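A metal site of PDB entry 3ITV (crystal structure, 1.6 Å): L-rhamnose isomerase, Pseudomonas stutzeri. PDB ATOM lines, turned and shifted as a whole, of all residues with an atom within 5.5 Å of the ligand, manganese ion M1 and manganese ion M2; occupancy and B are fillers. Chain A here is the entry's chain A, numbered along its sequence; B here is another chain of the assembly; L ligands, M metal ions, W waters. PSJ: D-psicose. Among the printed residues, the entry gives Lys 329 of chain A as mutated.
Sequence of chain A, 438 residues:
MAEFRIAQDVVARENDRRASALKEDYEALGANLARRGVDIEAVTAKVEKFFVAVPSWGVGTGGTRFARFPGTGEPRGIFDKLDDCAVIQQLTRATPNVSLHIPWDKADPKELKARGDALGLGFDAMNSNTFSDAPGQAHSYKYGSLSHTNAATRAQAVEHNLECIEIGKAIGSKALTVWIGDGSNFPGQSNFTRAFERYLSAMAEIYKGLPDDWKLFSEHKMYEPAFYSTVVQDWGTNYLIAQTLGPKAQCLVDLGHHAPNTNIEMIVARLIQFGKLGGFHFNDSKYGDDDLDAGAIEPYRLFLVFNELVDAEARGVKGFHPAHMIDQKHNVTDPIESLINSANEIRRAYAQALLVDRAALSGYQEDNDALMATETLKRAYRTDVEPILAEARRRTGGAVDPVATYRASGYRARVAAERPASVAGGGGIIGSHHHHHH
Merely in contact with manganese ion M2: Lys 221 (3.7 Å) and Asp 291 (3.95 Å).
Of the 21 residues printed, 5 come within 4 Å of manganese ion M2.
Along chain A the residues within 4 Å of manganese ion M2 span positions 221 to 291.
The nearest printed residue that does not touch manganese ion M2 is Asp 327 (4.4 Å).
Water W2 lies within hydrogen-bond range of the side-chain amino group of Lys 329, the side-chain carboxylate of Asp 291 and an oxygen (O5) of the ligand.
Water W3 bridges the side-chain carboxylate (OD1) of Asp 289 (2.4 Å) and the side-chain carboxylate (OD2) of Asp 291 (3.4 Å).
Water W1 lies within hydrogen-bond range of O4 of the ligand and OD1 of Asn 127.
OD1 of Asp 327 lies within hydrogen-bond range of NE1 of Trp 57 (3.0 Å).
ND2 of Asn 283 sits at hydrogen-bond distance from OD1 of Asp 254, 2.8 Å away.
The side-chain amino group (NZ) of Lys 221 is in salt-bridge range of the side-chain carboxylate (OE1) of Glu 224 (3.1 Å).
The side-chain amino group of Lys 329 is in salt-bridge range of the side-chain carboxylate of Asp 291.
The side-chain carboxylate (OD2) of Asp 289 sits close to the side-chain amino group (NZ) of Lys 221 (3.1 Å).
The guanidinium group (NH2) of Arg 65 of chain B is in hydrogen-bond range of the backbone carbonyl oxygen (O) of Asp 289 (3.1 Å).
The side-chain carboxylate (OD1) of Asp 327 is in salt-bridge range of the side-chain amino group (NZ) of Lys 329, 2.7 Å away.
The backbone carbonyl oxygen of Asp 327 is in hydrogen-bond range of the side-chain amide nitrogen of Asn 283 (2.9 Å).
O1 of the ligand sits close to NZ of Lys 221, at 2.7 Å.
A ring nitrogen (NE2) of His 101 is in hydrogen-bond range of an oxygen (O4) of the ligand, 3.1 Å away.
O5 of the ligand sits at hydrogen-bond distance from NZ of Lys 329, 2.6 Å away.
The side-chain carboxylate (OD2) of Asp 327 is bound to manganese ion M1.
Manganese ion M1 is bound by OE2 of Glu 219, 2.1 Å away.
Manganese ion M1 is bound by OD2 of Asp 254.
Manganese ion M1 is bound by an oxygen (O2) of the ligand (2.2 Å).
Manganese ion M1 is bound by a ring nitrogen (ND1) of His 281 (2.3 Å).
An oxygen (O3) of the ligand binds manganese ion M1, at 2.3 Å.
Manganese ion M1 has six donor atoms within binding distance.
Residues that only touch the ligand: Phe 66 of chain B (3.4 Å), Trp 179 (3.4 Å), Trp 57 (3.7 Å) and Trp 104 (3.96 Å).
13 residues have an atom within 4 Å of the ligand: Trp 57, His 101, Trp 104, Trp 179, Glu 219, Lys 221, Asp 254, His 257, His 281, Asp 289, Asp 327, Lys 329 and Phe 66 of chain B.
Of the 21 residues printed, 5 come within 4 Å of manganese ion M1.
The nearest printed residue that does not touch manganese ion M1 is Leu 252 (5.0 Å).
Manganese ion M2 is bound by water W3.
Manganese ion M2 is bound by O1 of the ligand.
NE2 of His 257 binds manganese ion M2 (2.0 Å).
Water W2 binds manganese ion M2 (2.1 Å).
OD2 of Asp 289 binds manganese ion M2, at 2.1 Å.
Manganese ion M2 is bound by O2 of the ligand (2.3 Å).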
ATOM      1  N   TRP A  57      20.341   6.936  20.243  1.00  0.00           N
ATOM      2  CA  TRP A  57      19.663   7.927  19.428  1.00  0.00           C
ATOM      3  C   TRP A  57      18.908   8.985  20.237  1.00  0.00           C
ATOM      4  O   TRP A  57      18.372   9.939  19.672  1.00  0.00           O
ATOM      5  CB  TRP A  57      18.705   7.231  18.457  1.00  0.00           C
ATOM      6  CG  TRP A  57      17.605   6.463  19.108  1.00  0.00           C
ATOM      7  CD1 TRP A  57      16.370   6.921  19.460  1.00  0.00           C
ATOM      8  CD2 TRP A  57      17.638   5.082  19.493  1.00  0.00           C
ATOM      9  NE1 TRP A  57      15.628   5.914  20.029  1.00  0.00           N
ATOM     10  CE2 TRP A  57      16.381   4.773  20.070  1.00  0.00           C
ATOM     11  CE3 TRP A  57      18.604   4.071  19.410  1.00  0.00           C
ATOM     12  CZ2 TRP A  57      16.065   3.505  20.547  1.00  0.00           C
ATOM     13  CZ3 TRP A  57      18.296   2.805  19.893  1.00  0.00           C
ATOM     14  CH2 TRP A  57      17.038   2.530  20.459  1.00  0.00           C
ATOM     15  N   HIS A 101      21.874   1.544  17.415  1.00  0.00           N
ATOM     16  CA  HIS A 101      21.017   1.528  16.236  1.00  0.00           C
ATOM     17  C   HIS A 101      21.939   1.537  15.015  1.00  0.00           C
ATOM     18  O   HIS A 101      22.791   2.402  14.887  1.00  0.00           O
ATOM     19  CB  HIS A 101      20.097   2.743  16.232  1.00  0.00           C
ATOM     20  CG  HIS A 101      18.718   2.471  15.705  1.00  0.00           C
ATOM     21  ND1 HIS A 101      18.496   2.069  14.406  1.00  0.00           N
ATOM     22  CD2 HIS A 101      17.514   2.510  16.311  1.00  0.00           C
ATOM     23  CE1 HIS A 101      17.196   1.877  14.236  1.00  0.00           C
ATOM     24  NE2 HIS A 101      16.576   2.136  15.374  1.00  0.00           N
ATOM     25  N   TRP A 104      23.199   3.983  12.073  1.00  0.00           N
ATOM     26  CA  TRP A 104      23.561   5.235  12.720  1.00  0.00           C
ATOM     27  C   TRP A 104      24.836   5.097  13.544  1.00  0.00           C
ATOM     28  O   TRP A 104      25.726   5.938  13.482  1.00  0.00           O
ATOM     29  CB  TRP A 104      22.447   5.754  13.644  1.00  0.00           C
ATOM     30  CG  TRP A 104      21.164   6.109  12.956  1.00  0.00           C
ATOM     31  CD1 TRP A 104      21.004   6.468  11.646  1.00  0.00           C
ATOM     32  CD2 TRP A 104      19.864   6.177  13.554  1.00  0.00           C
ATOM     33  NE1 TRP A 104      19.677   6.752  11.396  1.00  0.00           N
ATOM     34  CE2 TRP A 104      18.959   6.569  12.554  1.00  0.00           C
ATOM     35  CE3 TRP A 104      19.382   5.928  14.855  1.00  0.00           C
ATOM     36  CZ2 TRP A 104      17.587   6.738  12.800  1.00  0.00           C
ATOM     37  CZ3 TRP A 104      18.014   6.090  15.096  1.00  0.00           C
ATOM     38  CH2 TRP A 104      17.139   6.483  14.065  1.00  0.00           C
ATOM     39  N   ASN A 127      19.479  -2.649  17.319  1.00  0.00           N
ATOM     40  CA  ASN A 127      18.302  -2.168  16.608  1.00  0.00           C
ATOM     41  C   ASN A 127      18.658  -2.014  15.135  1.00  0.00           C
ATOM     42  O   ASN A 127      19.633  -1.344  14.790  1.00  0.00           O
ATOM     43  CB  ASN A 127      17.866  -0.806  17.170  1.00  0.00           C
ATOM     44  CG  ASN A 127      17.372  -0.884  18.591  1.00  0.00           C
ATOM     45  OD1 ASN A 127      16.173  -1.073  18.828  1.00  0.00           O
ATOM     46  ND2 ASN A 127      18.280  -0.771  19.550  1.00  0.00           N
ATOM     47  N   SER A 128      17.875  -2.645  14.265  1.00  0.00           N
ATOM     48  CA  SER A 128      18.094  -2.564  12.828  1.00  0.00           C
ATOM     49  C   SER A 128      17.346  -1.367  12.261  1.00  0.00           C
ATOM     50  O   SER A 128      16.413  -0.858  12.882  1.00  0.00           O
ATOM     51  CB  SER A 128      17.631  -3.855  12.147  1.00  0.00           C
ATOM     52  OG  SER A 128      16.272  -4.138  12.448  1.00  0.00           O
ATOM     53  N   PHE A 131      13.927   1.483   7.711  1.00  0.00           N
ATOM     54  CA  PHE A 131      12.844   2.440   7.593  1.00  0.00           C
ATOM     55  C   PHE A 131      13.381   3.730   6.975  1.00  0.00           C
ATOM     56  O   PHE A 131      12.700   4.751   6.932  1.00  0.00           O
ATOM     57  CB  PHE A 131      12.185   2.705   8.955  1.00  0.00           C
ATOM     58  CG  PHE A 131      13.148   3.058  10.055  1.00  0.00           C
ATOM     59  CD1 PHE A 131      13.666   4.343  10.168  1.00  0.00           C
ATOM     60  CD2 PHE A 131      13.515   2.104  11.005  1.00  0.00           C
ATOM     61  CE1 PHE A 131      14.537   4.676  11.214  1.00  0.00           C
ATOM     62  CE2 PHE A 131      14.378   2.422  12.048  1.00  0.00           C
ATOM     63  CZ  PHE A 131      14.891   3.711  12.149  1.00  0.00           C
ATOM     64  N   TRP A 179      12.022  -2.996  14.328  1.00  0.00           N
ATOM     65  CA  TRP A 179      10.887  -2.104  14.141  1.00  0.00           C
ATOM     66  C   TRP A 179      11.034  -1.570  12.728  1.00  0.00           C
ATOM     67  O   TRP A 179      12.102  -1.062  12.362  1.00  0.00           O
ATOM     68  CB  TRP A 179      10.876  -0.918  15.102  1.00  0.00           C
ATOM     69  CG  TRP A 179       9.787   0.057  14.709  1.00  0.00           C
ATOM     70  CD1 TRP A 179       8.443  -0.109  14.883  1.00  0.00           C
ATOM     71  CD2 TRP A 179       9.943   1.265  13.964  1.00  0.00           C
ATOM     72  NE1 TRP A 179       7.752   0.912  14.281  1.00  0.00           N
ATOM     73  CE2 TRP A 179       8.649   1.776  13.719  1.00  0.00           C
ATOM     74  CE3 TRP A 179      11.048   1.981  13.482  1.00  0.00           C
ATOM     75  CZ2 TRP A 179       8.430   2.964  12.998  1.00  0.00           C
ATOM     76  CZ3 TRP A 179      10.839   3.156  12.768  1.00  0.00           C
ATOM     77  CH2 TRP A 179       9.534   3.638  12.532  1.00  0.00           C
ATOM     78  N   GLU A 219       8.673  -5.124  17.239  1.00  0.00           N
ATOM     79  CA  GLU A 219       7.981  -3.997  17.877  1.00  0.00           C
ATOM     80  C   GLU A 219       6.790  -3.487  17.059  1.00  0.00           C
ATOM     81  O   GLU A 219       6.961  -3.002  15.942  1.00  0.00           O
ATOM     82  CB  GLU A 219       8.995  -2.869  18.103  1.00  0.00           C
ATOM     83  CG  GLU A 219       8.421  -1.583  18.666  1.00  0.00           C
ATOM     84  CD  GLU A 219       9.487  -0.536  18.933  1.00  0.00           C
ATOM     85  OE1 GLU A 219      10.638  -0.710  18.465  1.00  0.00           O
ATOM     86  OE2 GLU A 219       9.183   0.475  19.593  1.00  0.00           O
ATOM     87  N   LYS A 221       3.455  -1.053  16.125  1.00  0.00           N
ATOM     88  CA  LYS A 221       3.168   0.381  16.130  1.00  0.00           C
ATOM     89  C   LYS A 221       1.921   0.608  15.287  1.00  0.00           C
ATOM     90  O   LYS A 221       1.861   0.167  14.144  1.00  0.00           O
ATOM     91  CB  LYS A 221       4.347   1.168  15.558  1.00  0.00           C
ATOM     92  CG  LYS A 221       4.245   2.668  15.787  1.00  0.00           C
ATOM     93  CD  LYS A 221       5.480   3.401  15.299  1.00  0.00           C
ATOM     94  CE  LYS A 221       5.379   4.881  15.613  1.00  0.00           C
ATOM     95  NZ  LYS A 221       6.560   5.636  15.068  1.00  0.00           N
ATOM     96  N   GLU A 224       2.505   5.632  11.711  1.00  0.00           N
ATOM     97  CA  GLU A 224       3.689   6.483  11.568  1.00  0.00           C
ATOM     98  C   GLU A 224       4.944   5.618  11.464  1.00  0.00           C
ATOM     99  O   GLU A 224       5.346   4.972  12.425  1.00  0.00           O
ATOM    100  CB  GLU A 224       3.855   7.460  12.741  1.00  0.00           C
ATOM    101  CG  GLU A 224       5.023   8.425  12.486  1.00  0.00           C
ATOM    102  CD  GLU A 224       5.532   9.134  13.732  1.00  0.00           C
ATOM    103  OE1 GLU A 224       5.527   8.517  14.812  1.00  0.00           O
ATOM    104  OE2 GLU A 224       5.946  10.307  13.621  1.00  0.00           O
ATOM    105  N   LEU A 252       7.989  -6.695  21.734  1.00  0.00           N
ATOM    106  CA  LEU A 252       8.457  -5.526  22.472  1.00  0.00           C
ATOM    107  C   LEU A 252       7.323  -4.511  22.479  1.00  0.00           C
ATOM    108  O   LEU A 252       6.729  -4.215  21.446  1.00  0.00           O
ATOM    109  CB  LEU A 252       9.713  -4.938  21.820  1.00  0.00           C
ATOM    110  CG  LEU A 252      10.366  -3.803  22.595  1.00  0.00           C
ATOM    111  CD1 LEU A 252      11.884  -3.922  22.542  1.00  0.00           C
ATOM    112  CD2 LEU A 252       9.900  -2.480  22.044  1.00  0.00           C
ATOM    113  N   ASP A 254       6.217  -0.722  23.148  1.00  0.00           N
ATOM    114  CA  ASP A 254       6.628   0.675  23.243  1.00  0.00           C
ATOM    115  C   ASP A 254       5.355   1.388  23.671  1.00  0.00           C
ATOM    116  O   ASP A 254       4.356   1.375  22.950  1.00  0.00           O
ATOM    117  CB  ASP A 254       7.118   1.183  21.880  1.00  0.00           C
ATOM    118  CG  ASP A 254       7.644   2.600  21.952  1.00  0.00           C
ATOM    119  OD1 ASP A 254       6.929   3.474  22.478  1.00  0.00           O
ATOM    120  OD2 ASP A 254       8.771   2.866  21.472  1.00  0.00           O
ATOM    121  N   HIS A 257       2.939   3.525  21.285  1.00  0.00           N
ATOM    122  CA  HIS A 257       2.530   2.928  20.012  1.00  0.00           C
ATOM    123  C   HIS A 257       1.126   2.332  19.958  1.00  0.00           C
ATOM    124  O   HIS A 257       0.847   1.473  19.134  1.00  0.00           O
ATOM    125  CB  HIS A 257       3.527   1.843  19.621  1.00  0.00           C
ATOM    126  CG  HIS A 257       4.889   2.358  19.273  1.00  0.00           C
ATOM    127  ND1 HIS A 257       5.846   1.573  18.667  1.00  0.00           N
ATOM    128  CD2 HIS A 257       5.446   3.587  19.420  1.00  0.00           C
ATOM    129  CE1 HIS A 257       6.934   2.289  18.454  1.00  0.00           C
ATOM    130  NE2 HIS A 257       6.708   3.516  18.907  1.00  0.00           N
ATOM    131  N   HIS A 281       9.873  -0.369  25.703  1.00  0.00           N
ATOM    132  CA  HIS A 281      10.482   0.851  25.205  1.00  0.00           C
ATOM    133  C   HIS A 281       9.671   1.869  25.982  1.00  0.00           C
ATOM    134  O   HIS A 281       8.503   2.131  25.670  1.00  0.00           O
ATOM    135  CB  HIS A 281      10.272   1.024  23.705  1.00  0.00           C
ATOM    136  CG  HIS A 281      11.405   0.510  22.866  1.00  0.00           C
ATOM    137  ND1 HIS A 281      11.543   0.814  21.529  1.00  0.00           N
ATOM    138  CD2 HIS A 281      12.457  -0.293  23.183  1.00  0.00           C
ATOM    139  CE1 HIS A 281      12.628   0.221  21.059  1.00  0.00           C
ATOM    140  NE2 HIS A 281      13.203  -0.450  22.035  1.00  0.00           N
ATOM    141  N   ASN A 283       8.600   5.512  27.600  1.00  0.00           N
ATOM    142  CA  ASN A 283       8.460   6.913  27.208  1.00  0.00           C
ATOM    143  C   ASN A 283       7.055   7.306  27.633  1.00  0.00           C
ATOM    144  O   ASN A 283       6.308   6.474  28.168  1.00  0.00           O
ATOM    145  CB  ASN A 283       8.618   7.071  25.690  1.00  0.00           C
ATOM    146  CG  ASN A 283       7.774   6.086  24.887  1.00  0.00           C
ATOM    147  OD1 ASN A 283       6.552   6.030  25.057  1.00  0.00           O
ATOM    148  ND2 ASN A 283       8.414   5.306  24.017  1.00  0.00           N
ATOM    149  N   ASP A 289       2.692   8.970  19.128  1.00  0.00           N
ATOM    150  CA  ASP A 289       3.966   8.420  19.560  1.00  0.00           C
ATOM    151  C   ASP A 289       4.860   9.625  19.843  1.00  0.00           C
ATOM    152  O   ASP A 289       5.846   9.876  19.147  1.00  0.00           O
ATOM    153  CB  ASP A 289       4.567   7.538  18.472  1.00  0.00           C
ATOM    154  CG  ASP A 289       5.841   6.859  18.909  1.00  0.00           C
ATOM    155  OD1 ASP A 289       5.970   6.578  20.125  1.00  0.00           O
ATOM    156  OD2 ASP A 289       6.705   6.585  18.042  1.00  0.00           O
ATOM    157  N   ASP A 291       6.955  10.266  22.222  1.00  0.00           N
ATOM    158  CA  ASP A 291       8.305   9.970  22.716  1.00  0.00           C
ATOM    159  C   ASP A 291       8.818  10.919  23.793  1.00  0.00           C
ATOM    160  O   ASP A 291      10.007  11.259  23.818  1.00  0.00           O
ATOM    161  CB  ASP A 291       9.290   9.930  21.543  1.00  0.00           C
ATOM    162  CG  ASP A 291       9.116   8.699  20.670  1.00  0.00           C
ATOM    163  OD1 ASP A 291       8.871   7.617  21.242  1.00  0.00           O
ATOM    164  OD2 ASP A 291       9.213   8.808  19.431  1.00  0.00           O
ATOM    165  N   ASP A 327      13.017   4.616  25.094  1.00  0.00           N
ATOM    166  CA  ASP A 327      13.002   4.999  23.688  1.00  0.00           C
ATOM    167  C   ASP A 327      12.311   6.345  23.669  1.00  0.00           C
ATOM    168  O   ASP A 327      11.091   6.430  23.629  1.00  0.00           O
ATOM    169  CB  ASP A 327      12.226   4.015  22.810  1.00  0.00           C
ATOM    170  CG  ASP A 327      12.244   4.424  21.341  1.00  0.00           C
ATOM    171  OD1 ASP A 327      12.833   5.475  21.017  1.00  0.00           O
ATOM    172  OD2 ASP A 327      11.663   3.688  20.505  1.00  0.00           O
ATOM    173  N   LYS A 329      12.761  10.799  22.495  1.00  0.00           N
ATOM    174  CA  LYS A 329      13.368  11.807  21.656  1.00  0.00           C
ATOM    175  C   LYS A 329      13.216  13.086  22.465  1.00  0.00           C
ATOM    176  O   LYS A 329      12.141  13.365  23.008  1.00  0.00           O
ATOM    177  CB  LYS A 329      12.652  11.935  20.309  1.00  0.00           C
ATOM    178  CG  LYS A 329      12.944  10.801  19.333  1.00  0.00           C
ATOM    179  CD  LYS A 329      12.321   9.494  19.784  1.00  0.00           C
ATOM    180  CE  LYS A 329      12.542   8.394  18.756  1.00  0.00           C
ATOM    181  NZ  LYS A 329      11.789   7.168  19.119  1.00  0.00           N
ATOM    182  N   ARG B  65       9.378  12.163  10.184  1.00  0.00           N
ATOM    183  CA  ARG B  65      10.575  12.391  10.975  1.00  0.00           C
ATOM    184  C   ARG B  65      11.553  11.230  10.822  1.00  0.00           C
ATOM    185  O   ARG B  65      12.722  11.335  11.204  1.00  0.00           O
ATOM    186  CB  ARG B  65      10.240  12.585  12.450  1.00  0.00           C
ATOM    187  CG  ARG B  65       9.431  11.450  13.057  1.00  0.00           C
ATOM    188  CD  ARG B  65       9.278  11.638  14.567  1.00  0.00           C
ATOM    189  NE  ARG B  65       8.404  10.627  15.139  1.00  0.00           N
ATOM    190  CZ  ARG B  65       8.551  10.110  16.348  1.00  0.00           C
ATOM    191  NH1 ARG B  65       9.553  10.496  17.133  1.00  0.00           N
ATOM    192  NH2 ARG B  65       7.708   9.180  16.780  1.00  0.00           N
ATOM    193  N   PHE B  66      11.084  10.122  10.247  1.00  0.00           N
ATOM    194  CA  PHE B  66      11.925   8.945  10.053  1.00  0.00           C
ATOM    195  C   PHE B  66      12.705   8.968   8.747  1.00  0.00           C
ATOM    196  O   PHE B  66      13.854   8.511   8.698  1.00  0.00           O
ATOM    197  CB  PHE B  66      11.081   7.679  10.124  1.00  0.00           C
ATOM    198  CG  PHE B  66      10.515   7.411  11.475  1.00  0.00           C
ATOM    199  CD1 PHE B  66      11.344   6.997  12.512  1.00  0.00           C
ATOM    200  CD2 PHE B  66       9.164   7.612  11.733  1.00  0.00           C
ATOM    201  CE1 PHE B  66      10.836   6.801  13.797  1.00  0.00           C
ATOM    202  CE2 PHE B  66       8.651   7.421  13.006  1.00  0.00           C
ATOM    203  CZ  PHE B  66       9.491   7.016  14.041  1.00  0.00           C
HETATM  204  C1  PSJ L   1       9.723   4.000  16.096  1.00  0.00           C
HETATM  205  O1  PSJ L   1       8.684   4.874  16.510  1.00  0.00           O
HETATM  206  C2  PSJ L   1      10.237   3.224  17.293  1.00  0.00           C
HETATM  207  O2  PSJ L   1       9.705   3.347  18.389  1.00  0.00           O
HETATM  208  C3  PSJ L   1      11.411   2.260  17.119  1.00  0.00           C
HETATM  209  O3  PSJ L   1      11.762   1.698  18.377  1.00  0.00           O
HETATM  210  C4  PSJ L   1      12.615   2.998  16.522  1.00  0.00           C
HETATM  211  O4  PSJ L   1      13.608   2.049  16.132  1.00  0.00           O
HETATM  212  C5  PSJ L   1      13.209   3.997  17.505  1.00  0.00           C
HETATM  213  O5  PSJ L   1      12.193   4.848  18.008  1.00  0.00           O
HETATM  214  C6  PSJ L   1      14.276   4.834  16.806  1.00  0.00           C
HETATM  215  O6  PSJ L   1      13.677   5.619  15.789  1.00  0.00           O
HETATM  216 MN    MN M   1      10.383   2.146  20.134  1.00  0.00          MN
HETATM  217 MN    MN M   2       8.065   4.970  18.420  1.00  0.00          MN
HETATM  218  O   HOH W   1      14.159  -0.349  17.114  1.00  0.00           O
HETATM  219  O   HOH W   2       9.636   6.394  18.161  1.00  0.00           O
HETATM  220  O   HOH W   3       8.232   5.647  20.056  1.00  0.00           O
